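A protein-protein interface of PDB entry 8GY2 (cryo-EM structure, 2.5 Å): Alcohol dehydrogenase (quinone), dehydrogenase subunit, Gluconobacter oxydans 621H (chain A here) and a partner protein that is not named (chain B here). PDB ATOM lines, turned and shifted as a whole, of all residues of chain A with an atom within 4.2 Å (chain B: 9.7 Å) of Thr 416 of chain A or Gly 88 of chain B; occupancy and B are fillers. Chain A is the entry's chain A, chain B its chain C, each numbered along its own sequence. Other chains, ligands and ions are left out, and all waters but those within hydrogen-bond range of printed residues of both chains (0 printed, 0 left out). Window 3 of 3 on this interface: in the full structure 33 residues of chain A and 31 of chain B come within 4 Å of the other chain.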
ATOM      1  N   LYS A 304      24.440 -12.282 -35.821  1.00  0.00           N
ATOM      2  CA  LYS A 304      23.110 -12.076 -35.256  1.00  0.00           C
ATOM      3  C   LYS A 304      22.090 -11.772 -36.343  1.00  0.00           C
ATOM      4  O   LYS A 304      20.969 -12.294 -36.317  1.00  0.00           O
ATOM      5  CB  LYS A 304      23.150 -10.943 -34.233  1.00  0.00           C
ATOM      6  CG  LYS A 304      22.108 -11.022 -33.141  1.00  0.00           C
ATOM      7  CD  LYS A 304      22.107  -9.737 -32.337  1.00  0.00           C
ATOM      8  CE  LYS A 304      22.571  -9.975 -30.915  1.00  0.00           C
ATOM      9  NZ  LYS A 304      22.819  -8.695 -30.202  1.00  0.00           N
ATOM     10  N   PRO A 409      35.486 -14.163 -25.621  1.00  0.00           N
ATOM     11  CA  PRO A 409      34.107 -13.643 -25.650  1.00  0.00           C
ATOM     12  C   PRO A 409      33.968 -12.315 -26.370  1.00  0.00           C
ATOM     13  O   PRO A 409      32.934 -12.071 -27.003  1.00  0.00           O
ATOM     14  CB  PRO A 409      33.740 -13.514 -24.166  1.00  0.00           C
ATOM     15  CG  PRO A 409      34.729 -14.323 -23.416  1.00  0.00           C
ATOM     16  CD  PRO A 409      35.882 -14.673 -24.299  1.00  0.00           C
ATOM     17  N   LEU A 412      33.468 -12.179 -30.456  1.00  0.00           N
ATOM     18  CA  LEU A 412      32.115 -12.244 -30.988  1.00  0.00           C
ATOM     19  C   LEU A 412      31.445 -10.890 -30.812  1.00  0.00           C
ATOM     20  O   LEU A 412      30.516 -10.746 -30.011  1.00  0.00           O
ATOM     21  CB  LEU A 412      31.315 -13.347 -30.295  1.00  0.00           C
ATOM     22  CG  LEU A 412      32.041 -14.685 -30.143  1.00  0.00           C
ATOM     23  CD1 LEU A 412      31.373 -15.543 -29.084  1.00  0.00           C
ATOM     24  CD2 LEU A 412      32.099 -15.419 -31.471  1.00  0.00           C
ATOM     25  N   TRP A 413      31.924  -9.891 -31.560  1.00  0.00           N
ATOM     26  CA  TRP A 413      31.401  -8.534 -31.434  1.00  0.00           C
ATOM     27  C   TRP A 413      29.914  -8.479 -31.734  1.00  0.00           C
ATOM     28  O   TRP A 413      29.199  -7.630 -31.188  1.00  0.00           O
ATOM     29  CB  TRP A 413      32.151  -7.599 -32.381  1.00  0.00           C
ATOM     30  CG  TRP A 413      32.127  -8.062 -33.809  1.00  0.00           C
ATOM     31  CD1 TRP A 413      32.996  -8.928 -34.402  1.00  0.00           C
ATOM     32  CD2 TRP A 413      31.184  -7.686 -34.821  1.00  0.00           C
ATOM     33  NE1 TRP A 413      32.656  -9.115 -35.718  1.00  0.00           N
ATOM     34  CE2 TRP A 413      31.546  -8.364 -36.001  1.00  0.00           C
ATOM     35  CE3 TRP A 413      30.069  -6.844 -34.844  1.00  0.00           C
ATOM     36  CZ2 TRP A 413      30.836  -8.223 -37.191  1.00  0.00           C
ATOM     37  CZ3 TRP A 413      29.367  -6.706 -36.026  1.00  0.00           C
ATOM     38  CH2 TRP A 413      29.752  -7.392 -37.182  1.00  0.00           C
ATOM     39  N   THR A 414      29.436  -9.364 -32.605  1.00  0.00           N
ATOM     40  CA  THR A 414      28.028  -9.355 -32.975  1.00  0.00           C
ATOM     41  C   THR A 414      27.146  -9.707 -31.783  1.00  0.00           C
ATOM     42  O   THR A 414      26.076  -9.119 -31.595  1.00  0.00           O
ATOM     43  CB  THR A 414      27.798 -10.323 -34.130  1.00  0.00           C
ATOM     44  OG1 THR A 414      28.757 -10.064 -35.161  1.00  0.00           O
ATOM     45  CG2 THR A 414      26.441 -10.106 -34.704  1.00  0.00           C
ATOM     46  N   LEU A 415      27.578 -10.673 -30.969  1.00  0.00           N
ATOM     47  CA  LEU A 415      26.827 -11.040 -29.774  1.00  0.00           C
ATOM     48  C   LEU A 415      26.992 -10.013 -28.659  1.00  0.00           C
ATOM     49  O   LEU A 415      26.025  -9.694 -27.962  1.00  0.00           O
ATOM     50  CB  LEU A 415      27.257 -12.425 -29.293  1.00  0.00           C
ATOM     51  CG  LEU A 415      27.182 -13.544 -30.334  1.00  0.00           C
ATOM     52  CD1 LEU A 415      27.583 -14.875 -29.723  1.00  0.00           C
ATOM     53  CD2 LEU A 415      25.787 -13.627 -30.926  1.00  0.00           C
ATOM     54  N   THR A 416      28.207  -9.493 -28.468  1.00  0.00           N
ATOM     55  CA  THR A 416      28.437  -8.524 -27.400  1.00  0.00           C
ATOM     56  C   THR A 416      27.876  -7.150 -27.734  1.00  0.00           C
ATOM     57  O   THR A 416      27.564  -6.376 -26.823  1.00  0.00           O
ATOM     58  CB  THR A 416      29.933  -8.399 -27.099  1.00  0.00           C
ATOM     59  OG1 THR A 416      30.629  -7.989 -28.282  1.00  0.00           O
ATOM     60  CG2 THR A 416      30.496  -9.722 -26.618  1.00  0.00           C
ATOM     61  N   GLY A 417      27.742  -6.828 -29.018  1.00  0.00           N
ATOM     62  CA  GLY A 417      27.285  -5.510 -29.410  1.00  0.00           C
ATOM     63  C   GLY A 417      28.246  -4.394 -29.069  1.00  0.00           C
ATOM     64  O   GLY A 417      27.809  -3.288 -28.737  1.00  0.00           O
ATOM     65  N   LYS A 418      29.546  -4.655 -29.141  1.00  0.00           N
ATOM     66  CA  LYS A 418      30.580  -3.672 -28.871  1.00  0.00           C
ATOM     67  C   LYS A 418      31.627  -3.721 -29.973  1.00  0.00           C
ATOM     68  O   LYS A 418      31.852  -4.777 -30.572  1.00  0.00           O
ATOM     69  CB  LYS A 418      31.249  -3.927 -27.512  1.00  0.00           C
ATOM     70  CG  LYS A 418      30.690  -3.082 -26.378  1.00  0.00           C
ATOM     71  CD  LYS A 418      30.382  -3.920 -25.143  1.00  0.00           C
ATOM     72  CE  LYS A 418      31.355  -5.079 -24.986  1.00  0.00           C
ATOM     73  NZ  LYS A 418      31.238  -5.730 -23.652  1.00  0.00           N
ATOM     74  N   ALA B  49      20.710 -15.779 -20.131  1.00  0.00           N
ATOM     75  CA  ALA B  49      21.479 -15.255 -21.257  1.00  0.00           C
ATOM     76  C   ALA B  49      22.928 -15.718 -21.185  1.00  0.00           C
ATOM     77  O   ALA B  49      23.703 -15.501 -22.121  1.00  0.00           O
ATOM     78  CB  ALA B  49      21.395 -13.728 -21.325  1.00  0.00           C
ATOM     79  N   SER B  77      16.523 -17.486 -24.700  1.00  0.00           N
ATOM     80  CA  SER B  77      17.016 -16.301 -25.384  1.00  0.00           C
ATOM     81  C   SER B  77      15.901 -15.366 -25.832  1.00  0.00           C
ATOM     82  O   SER B  77      16.192 -14.261 -26.300  1.00  0.00           O
ATOM     83  CB  SER B  77      17.856 -16.707 -26.599  1.00  0.00           C
ATOM     84  OG  SER B  77      17.601 -15.854 -27.700  1.00  0.00           O
ATOM     85  N   TYR B  80      14.287 -13.886 -21.864  1.00  0.00           N
ATOM     86  CA  TYR B  80      15.245 -13.017 -21.195  1.00  0.00           C
ATOM     87  C   TYR B  80      16.017 -12.127 -22.161  1.00  0.00           C
ATOM     88  O   TYR B  80      16.943 -11.430 -21.735  1.00  0.00           O
ATOM     89  CB  TYR B  80      16.209 -13.857 -20.359  1.00  0.00           C
ATOM     90  CG  TYR B  80      15.537 -14.550 -19.197  1.00  0.00           C
ATOM     91  CD1 TYR B  80      15.325 -13.885 -17.997  1.00  0.00           C
ATOM     92  CD2 TYR B  80      15.111 -15.866 -19.301  1.00  0.00           C
ATOM     93  CE1 TYR B  80      14.708 -14.514 -16.934  1.00  0.00           C
ATOM     94  CE2 TYR B  80      14.494 -16.503 -18.243  1.00  0.00           C
ATOM     95  CZ  TYR B  80      14.296 -15.822 -17.061  1.00  0.00           C
ATOM     96  OH  TYR B  80      13.682 -16.451 -16.004  1.00  0.00           O
ATOM     97  N   LYS B  81      15.660 -12.140 -23.446  1.00  0.00           N
ATOM     98  CA  LYS B  81      16.193 -11.206 -24.440  1.00  0.00           C
ATOM     99  C   LYS B  81      17.719 -11.288 -24.526  1.00  0.00           C
ATOM    100  O   LYS B  81      18.440 -10.330 -24.240  1.00  0.00           O
ATOM    101  CB  LYS B  81      15.732  -9.777 -24.135  1.00  0.00           C
ATOM    102  CG  LYS B  81      14.255  -9.540 -24.390  1.00  0.00           C
ATOM    103  CD  LYS B  81      13.713  -8.432 -23.505  1.00  0.00           C
ATOM    104  CE  LYS B  81      12.202  -8.313 -23.629  1.00  0.00           C
ATOM    105  NZ  LYS B  81      11.639  -9.307 -24.585  1.00  0.00           N
ATOM    106  N   ALA B  82      18.204 -12.462 -24.932  1.00  0.00           N
ATOM    107  CA  ALA B  82      19.646 -12.663 -25.029  1.00  0.00           C
ATOM    108  C   ALA B  82      20.232 -11.951 -26.243  1.00  0.00           C
ATOM    109  O   ALA B  82      21.308 -11.349 -26.153  1.00  0.00           O
ATOM    110  CB  ALA B  82      19.969 -14.155 -25.076  1.00  0.00           C
ATOM    111  N   THR B  83      19.549 -12.009 -27.387  1.00  0.00           N
ATOM    112  CA  THR B  83      20.068 -11.422 -28.620  1.00  0.00           C
ATOM    113  C   THR B  83      19.439 -10.067 -28.932  1.00  0.00           C
ATOM    114  O   THR B  83      20.142  -9.056 -29.008  1.00  0.00           O
ATOM    115  CB  THR B  83      19.845 -12.391 -29.789  1.00  0.00           C
ATOM    116  OG1 THR B  83      18.472 -12.346 -30.194  1.00  0.00           O
ATOM    117  CG2 THR B  83      20.200 -13.811 -29.377  1.00  0.00           C
ATOM    118  N   GLU B  84      18.121 -10.032 -29.123  1.00  0.00           N
ATOM    119  CA  GLU B  84      17.305  -8.838 -29.335  1.00  0.00           C
ATOM    120  C   GLU B  84      17.617  -8.097 -30.634  1.00  0.00           C
ATOM    121  O   GLU B  84      16.959  -7.089 -30.918  1.00  0.00           O
ATOM    122  CB  GLU B  84      17.413  -7.845 -28.170  1.00  0.00           C
ATOM    123  CG  GLU B  84      16.249  -7.912 -27.199  1.00  0.00           C
ATOM    124  CD  GLU B  84      14.952  -8.311 -27.875  1.00  0.00           C
ATOM    125  OE1 GLU B  84      14.368  -7.466 -28.587  1.00  0.00           O
ATOM    126  OE2 GLU B  84      14.516  -9.466 -27.695  1.00  0.00           O
ATOM    127  N   GLN B  85      18.611  -8.536 -31.410  1.00  0.00           N
ATOM    128  CA  GLN B  85      18.880  -8.044 -32.760  1.00  0.00           C
ATOM    129  C   GLN B  85      19.363  -6.595 -32.794  1.00  0.00           C
ATOM    130  O   GLN B  85      19.767  -6.099 -33.850  1.00  0.00           O
ATOM    131  CB  GLN B  85      17.632  -8.199 -33.637  1.00  0.00           C
ATOM    132  CG  GLN B  85      17.910  -8.273 -35.128  1.00  0.00           C
ATOM    133  CD  GLN B  85      18.235  -9.677 -35.592  1.00  0.00           C
ATOM    134  OE1 GLN B  85      18.206 -10.625 -34.808  1.00  0.00           O
ATOM    135  NE2 GLN B  85      18.549  -9.818 -36.874  1.00  0.00           N
ATOM    136  N   THR B  86      19.339  -5.909 -31.651  1.00  0.00           N
ATOM    137  CA  THR B  86      19.848  -4.544 -31.571  1.00  0.00           C
ATOM    138  C   THR B  86      20.556  -4.271 -30.251  1.00  0.00           C
ATOM    139  O   THR B  86      20.947  -3.124 -30.000  1.00  0.00           O
ATOM    140  CB  THR B  86      18.719  -3.524 -31.768  1.00  0.00           C
ATOM    141  OG1 THR B  86      17.473  -4.098 -31.354  1.00  0.00           O
ATOM    142  CG2 THR B  86      18.623  -3.106 -33.227  1.00  0.00           C
ATOM    143  N   VAL B  87      20.733  -5.285 -29.407  1.00  0.00           N
ATOM    144  CA  VAL B  87      21.163  -5.120 -28.029  1.00  0.00           C
ATOM    145  C   VAL B  87      22.403  -5.993 -27.836  1.00  0.00           C
ATOM    146  O   VAL B  87      22.746  -6.815 -28.686  1.00  0.00           O
ATOM    147  CB  VAL B  87      20.000  -5.462 -27.052  1.00  0.00           C
ATOM    148  CG1 VAL B  87      20.387  -5.487 -25.571  1.00  0.00           C
ATOM    149  CG2 VAL B  87      18.837  -4.503 -27.275  1.00  0.00           C
ATOM    150  N   GLY B  88      23.076  -5.809 -26.704  1.00  0.00           N
ATOM    151  CA  GLY B  88      24.360  -6.421 -26.438  1.00  0.00           C
ATOM    152  C   GLY B  88      24.203  -7.728 -25.693  1.00  0.00           C
ATOM    153  O   GLY B  88      24.043  -8.774 -26.327  1.00  0.00           O
ATOM    154  N   ASN B  89      24.269  -7.686 -24.360  1.00  0.00           N
ATOM    155  CA  ASN B  89      24.247  -8.889 -23.532  1.00  0.00           C
ATOM    156  C   ASN B  89      25.490  -9.737 -23.767  1.00  0.00           C
ATOM    157  O   ASN B  89      25.411 -10.851 -24.295  1.00  0.00           O
ATOM    158  CB  ASN B  89      22.979  -9.712 -23.785  1.00  0.00           C
ATOM    159  CG  ASN B  89      22.679 -10.672 -22.661  1.00  0.00           C
ATOM    160  OD1 ASN B  89      23.433 -11.612 -22.418  1.00  0.00           O
ATOM    161  ND2 ASN B  89      21.570 -10.444 -21.968  1.00  0.00           N
ATOM    162  N   PHE B  90      26.647  -9.180 -23.396  1.00  0.00           N
ATOM    163  CA  PHE B  90      27.917  -9.902 -23.420  1.00  0.00           C
ATOM    164  C   PHE B  90      27.816 -11.288 -22.791  1.00  0.00           C
ATOM    165  O   PHE B  90      28.610 -12.178 -23.122  1.00  0.00           O
ATOM    166  CB  PHE B  90      28.980  -9.056 -22.708  1.00  0.00           C
ATOM    167  CG  PHE B  90      30.145  -9.840 -22.173  1.00  0.00           C
ATOM    168  CD1 PHE B  90      31.229 -10.134 -22.980  1.00  0.00           C
ATOM    169  CD2 PHE B  90      30.168 -10.258 -20.852  1.00  0.00           C
ATOM    170  CE1 PHE B  90      32.303 -10.846 -22.487  1.00  0.00           C
ATOM    171  CE2 PHE B  90      31.239 -10.973 -20.355  1.00  0.00           C
ATOM    172  CZ  PHE B  90      32.308 -11.265 -21.174  1.00  0.00           C
ATOM    173  N   ASP B  91      26.856 -11.494 -21.886  1.00  0.00           N
ATOM    174  CA  ASP B  91      26.673 -12.804 -21.271  1.00  0.00           C
ATOM    175  C   ASP B  91      26.338 -13.887 -22.290  1.00  0.00           C
ATOM    176  O   ASP B  91      26.554 -15.069 -22.009  1.00  0.00           O
ATOM    177  CB  ASP B  91      25.576 -12.739 -20.208  1.00  0.00           C
ATOM    178  CG  ASP B  91      26.129 -12.536 -18.813  1.00  0.00           C
ATOM    179  OD1 ASP B  91      27.363 -12.426 -18.672  1.00  0.00           O
ATOM    180  OD2 ASP B  91      25.327 -12.486 -17.857  1.00  0.00           O
ATOM    181  N   TYR B  92      25.800 -13.520 -23.455  1.00  0.00           N
ATOM    182  CA  TYR B  92      25.554 -14.520 -24.489  1.00  0.00           C
ATOM    183  C   TYR B  92      26.862 -15.007 -25.100  1.00  0.00           C
ATOM    184  O   TYR B  92      27.068 -16.214 -25.272  1.00  0.00           O
ATOM    185  CB  TYR B  92      24.630 -13.953 -25.567  1.00  0.00           C
ATOM    186  CG  TYR B  92      24.026 -15.014 -26.457  1.00  0.00           C
ATOM    187  CD1 TYR B  92      23.068 -15.892 -25.971  1.00  0.00           C
ATOM    188  CD2 TYR B  92      24.418 -15.142 -27.782  1.00  0.00           C
ATOM    189  CE1 TYR B  92      22.515 -16.864 -26.779  1.00  0.00           C
ATOM    190  CE2 TYR B  92      23.871 -16.112 -28.597  1.00  0.00           C
ATOM    191  CZ  TYR B  92      22.920 -16.970 -28.091  1.00  0.00           C
ATOM    192  OH  TYR B  92      22.373 -17.936 -28.900  1.00  0.00           O
ATOM    193  N   ALA B  93      27.758 -14.077 -25.438  1.00  0.00           N
ATOM    194  CA  ALA B  93      29.070 -14.467 -25.942  1.00  0.00           C
ATOM    195  C   ALA B  93      29.855 -15.232 -24.885  1.00  0.00           C
ATOM    196  O   ALA B  93      30.533 -16.218 -25.196  1.00  0.00           O
ATOM    197  CB  ALA B  93      29.846 -13.236 -26.404  1.00  0.00           C
ATOM    198  N   LEU B  94      29.777 -14.791 -23.630  1.00  0.00           N
ATOM    199  CA  LEU B  94      30.369 -15.529 -22.516  1.00  0.00           C
ATOM    200  C   LEU B  94      29.448 -16.703 -22.200  1.00  0.00           C
ATOM    201  O   LEU B  94      28.599 -16.659 -21.307  1.00  0.00           O
ATOM    202  CB  LEU B  94      30.569 -14.628 -21.307  1.00  0.00           C
ATOM    203  CG  LEU B  94      31.330 -15.286 -20.159  1.00  0.00           C
ATOM    204  CD1 LEU B  94      32.809 -14.985 -20.286  1.00  0.00           C
ATOM    205  CD2 LEU B  94      30.793 -14.827 -18.815  1.00  0.00           C
ATOM    206  N   GLY B  95      29.645 -17.786 -22.940  1.00  0.00           N
ATOM    207  CA  GLY B  95      28.746 -18.918 -22.883  1.00  0.00           C
ATOM    208  C   GLY B  95      28.555 -19.523 -24.254  1.00  0.00           C
ATOM    209  O   GLY B  95      28.383 -20.737 -24.381  1.00  0.00           O
ATOM    210  N   THR B  96      28.604 -18.690 -25.296  1.00  0.00           N
ATOM    211  CA  THR B  96      28.782 -19.229 -26.638  1.00  0.00           C
ATOM    212  C   THR B  96      30.128 -19.930 -26.749  1.00  0.00           C
ATOM    213  O   THR B  96      30.251 -20.943 -27.448  1.00  0.00           O
ATOM    214  CB  THR B  96      28.652 -18.116 -27.676  1.00  0.00           C
ATOM    215  OG1 THR B  96      27.357 -17.514 -27.566  1.00  0.00           O
ATOM    216  CG2 THR B  96      28.809 -18.671 -29.076  1.00  0.00           C
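Of the 9 printed residues of chain A, 5 touch a printed residue of chain B.
Of the 19 printed residues of chain B, 10 touch a printed residue of chain A.
Among the printed residues, 15 pairs touch across the chains.
O of Leu 412 of chain A is in hydrogen-bond range of OG1 of Thr 416 of chain A (3.3 Å).
The side-chain hydroxyl (OG1) of Thr 416 of chain A lies within hydrogen-bond range of the backbone carbonyl oxygen (O) of Trp 413 of chain A, at 3.3 Å.
O of Ala 49 of chain B lies close to N of Tyr 92 of chain B (3.2 Å).
The backbone NH (N) of Asp 91 of chain B lies close to the side-chain amide oxygen (OD1) of Asn 89 of chain B (3.5 Å).
N of Tyr 92 of chain B sits at hydrogen-bond distance from OD1 of Asn 89 of chain B (3.2 Å).
O of Tyr 92 of chain B lies within hydrogen-bond range of OG1 of Thr 96 of chain B, at 2.7 Å.
Among the printed residues, pairs that only touch across the chains: Thr 416 of chain A with Gly 88 of chain B (3.2 Å), Pro 409 of chain A with Ala 93 of chain B (3.4 Å), Leu 415 of chain A with Thr 96 of chain B (3.4 Å), Pro 409 of chain A with Phe 90 of chain B (3.5 Å), Lys 304 of chain A with Gln 85 of chain B (3.5 Å), Thr 416 of chain A with Ala 93 of chain B (3.6 Å), Leu 415 of chain A with Tyr 92 of chain B (3.7 Å), Pro 409 of chain A with Leu 94 of chain B (3.7 Å), Thr 416 of chain A with Phe 90 of chain B (3.7 Å), Leu 412 of chain A with Ala 93 of chain B (3.9 Å), Leu 415 of chain A with Asn 89 of chain B (3.9 Å) and Leu 415 of chain A with Ala 93 of chain B (3.96 Å).
O of Thr 83 of chain B sits at hydrogen-bond distance from NZ of Lys 304 of chain A (3.0 Å).
O of Val 87 of chain B is in hydrogen-bond range of NZ of Lys 304 of chain A, at 2.4 Å.
O of Leu 415 of chain A sits close to O of Gly 88 of chain B, at 2.7 Å.
Of chain B, only Gly 88, Phe 90 and Ala 93 come within 4 Å of Thr 416 of chain A.
Printed residues of chain A within 4 Å of Gly 88 of chain B: Leu 415 and Thr 416.
Leu 415 of chain A touches just these residues of chain B: Gly 88 (2.7 Å), Asn 89 (3.9 Å), Tyr 92 (3.7 Å), Ala 93 (3.96 Å) and Thr 96 (3.4 Å).
Gly 417 of chain A touches none of the printed residues of chain B.
Of the printed residues of chain A, Tyr 92 of chain B touches Leu 415 (3.7 Å).
Printed residues of chain B within 4 Å of Pro 409 of chain A: Phe 90 (3.5 Å), Ala 93 (3.4 Å) and Leu 94 (3.7 Å).
Of the printed residues of chain A, Thr 83 of chain B touches Lys 304.
The nearest residue of chain B that does not touch Thr 416 of chain A is Asn 89 of chain B (4.3 Å).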
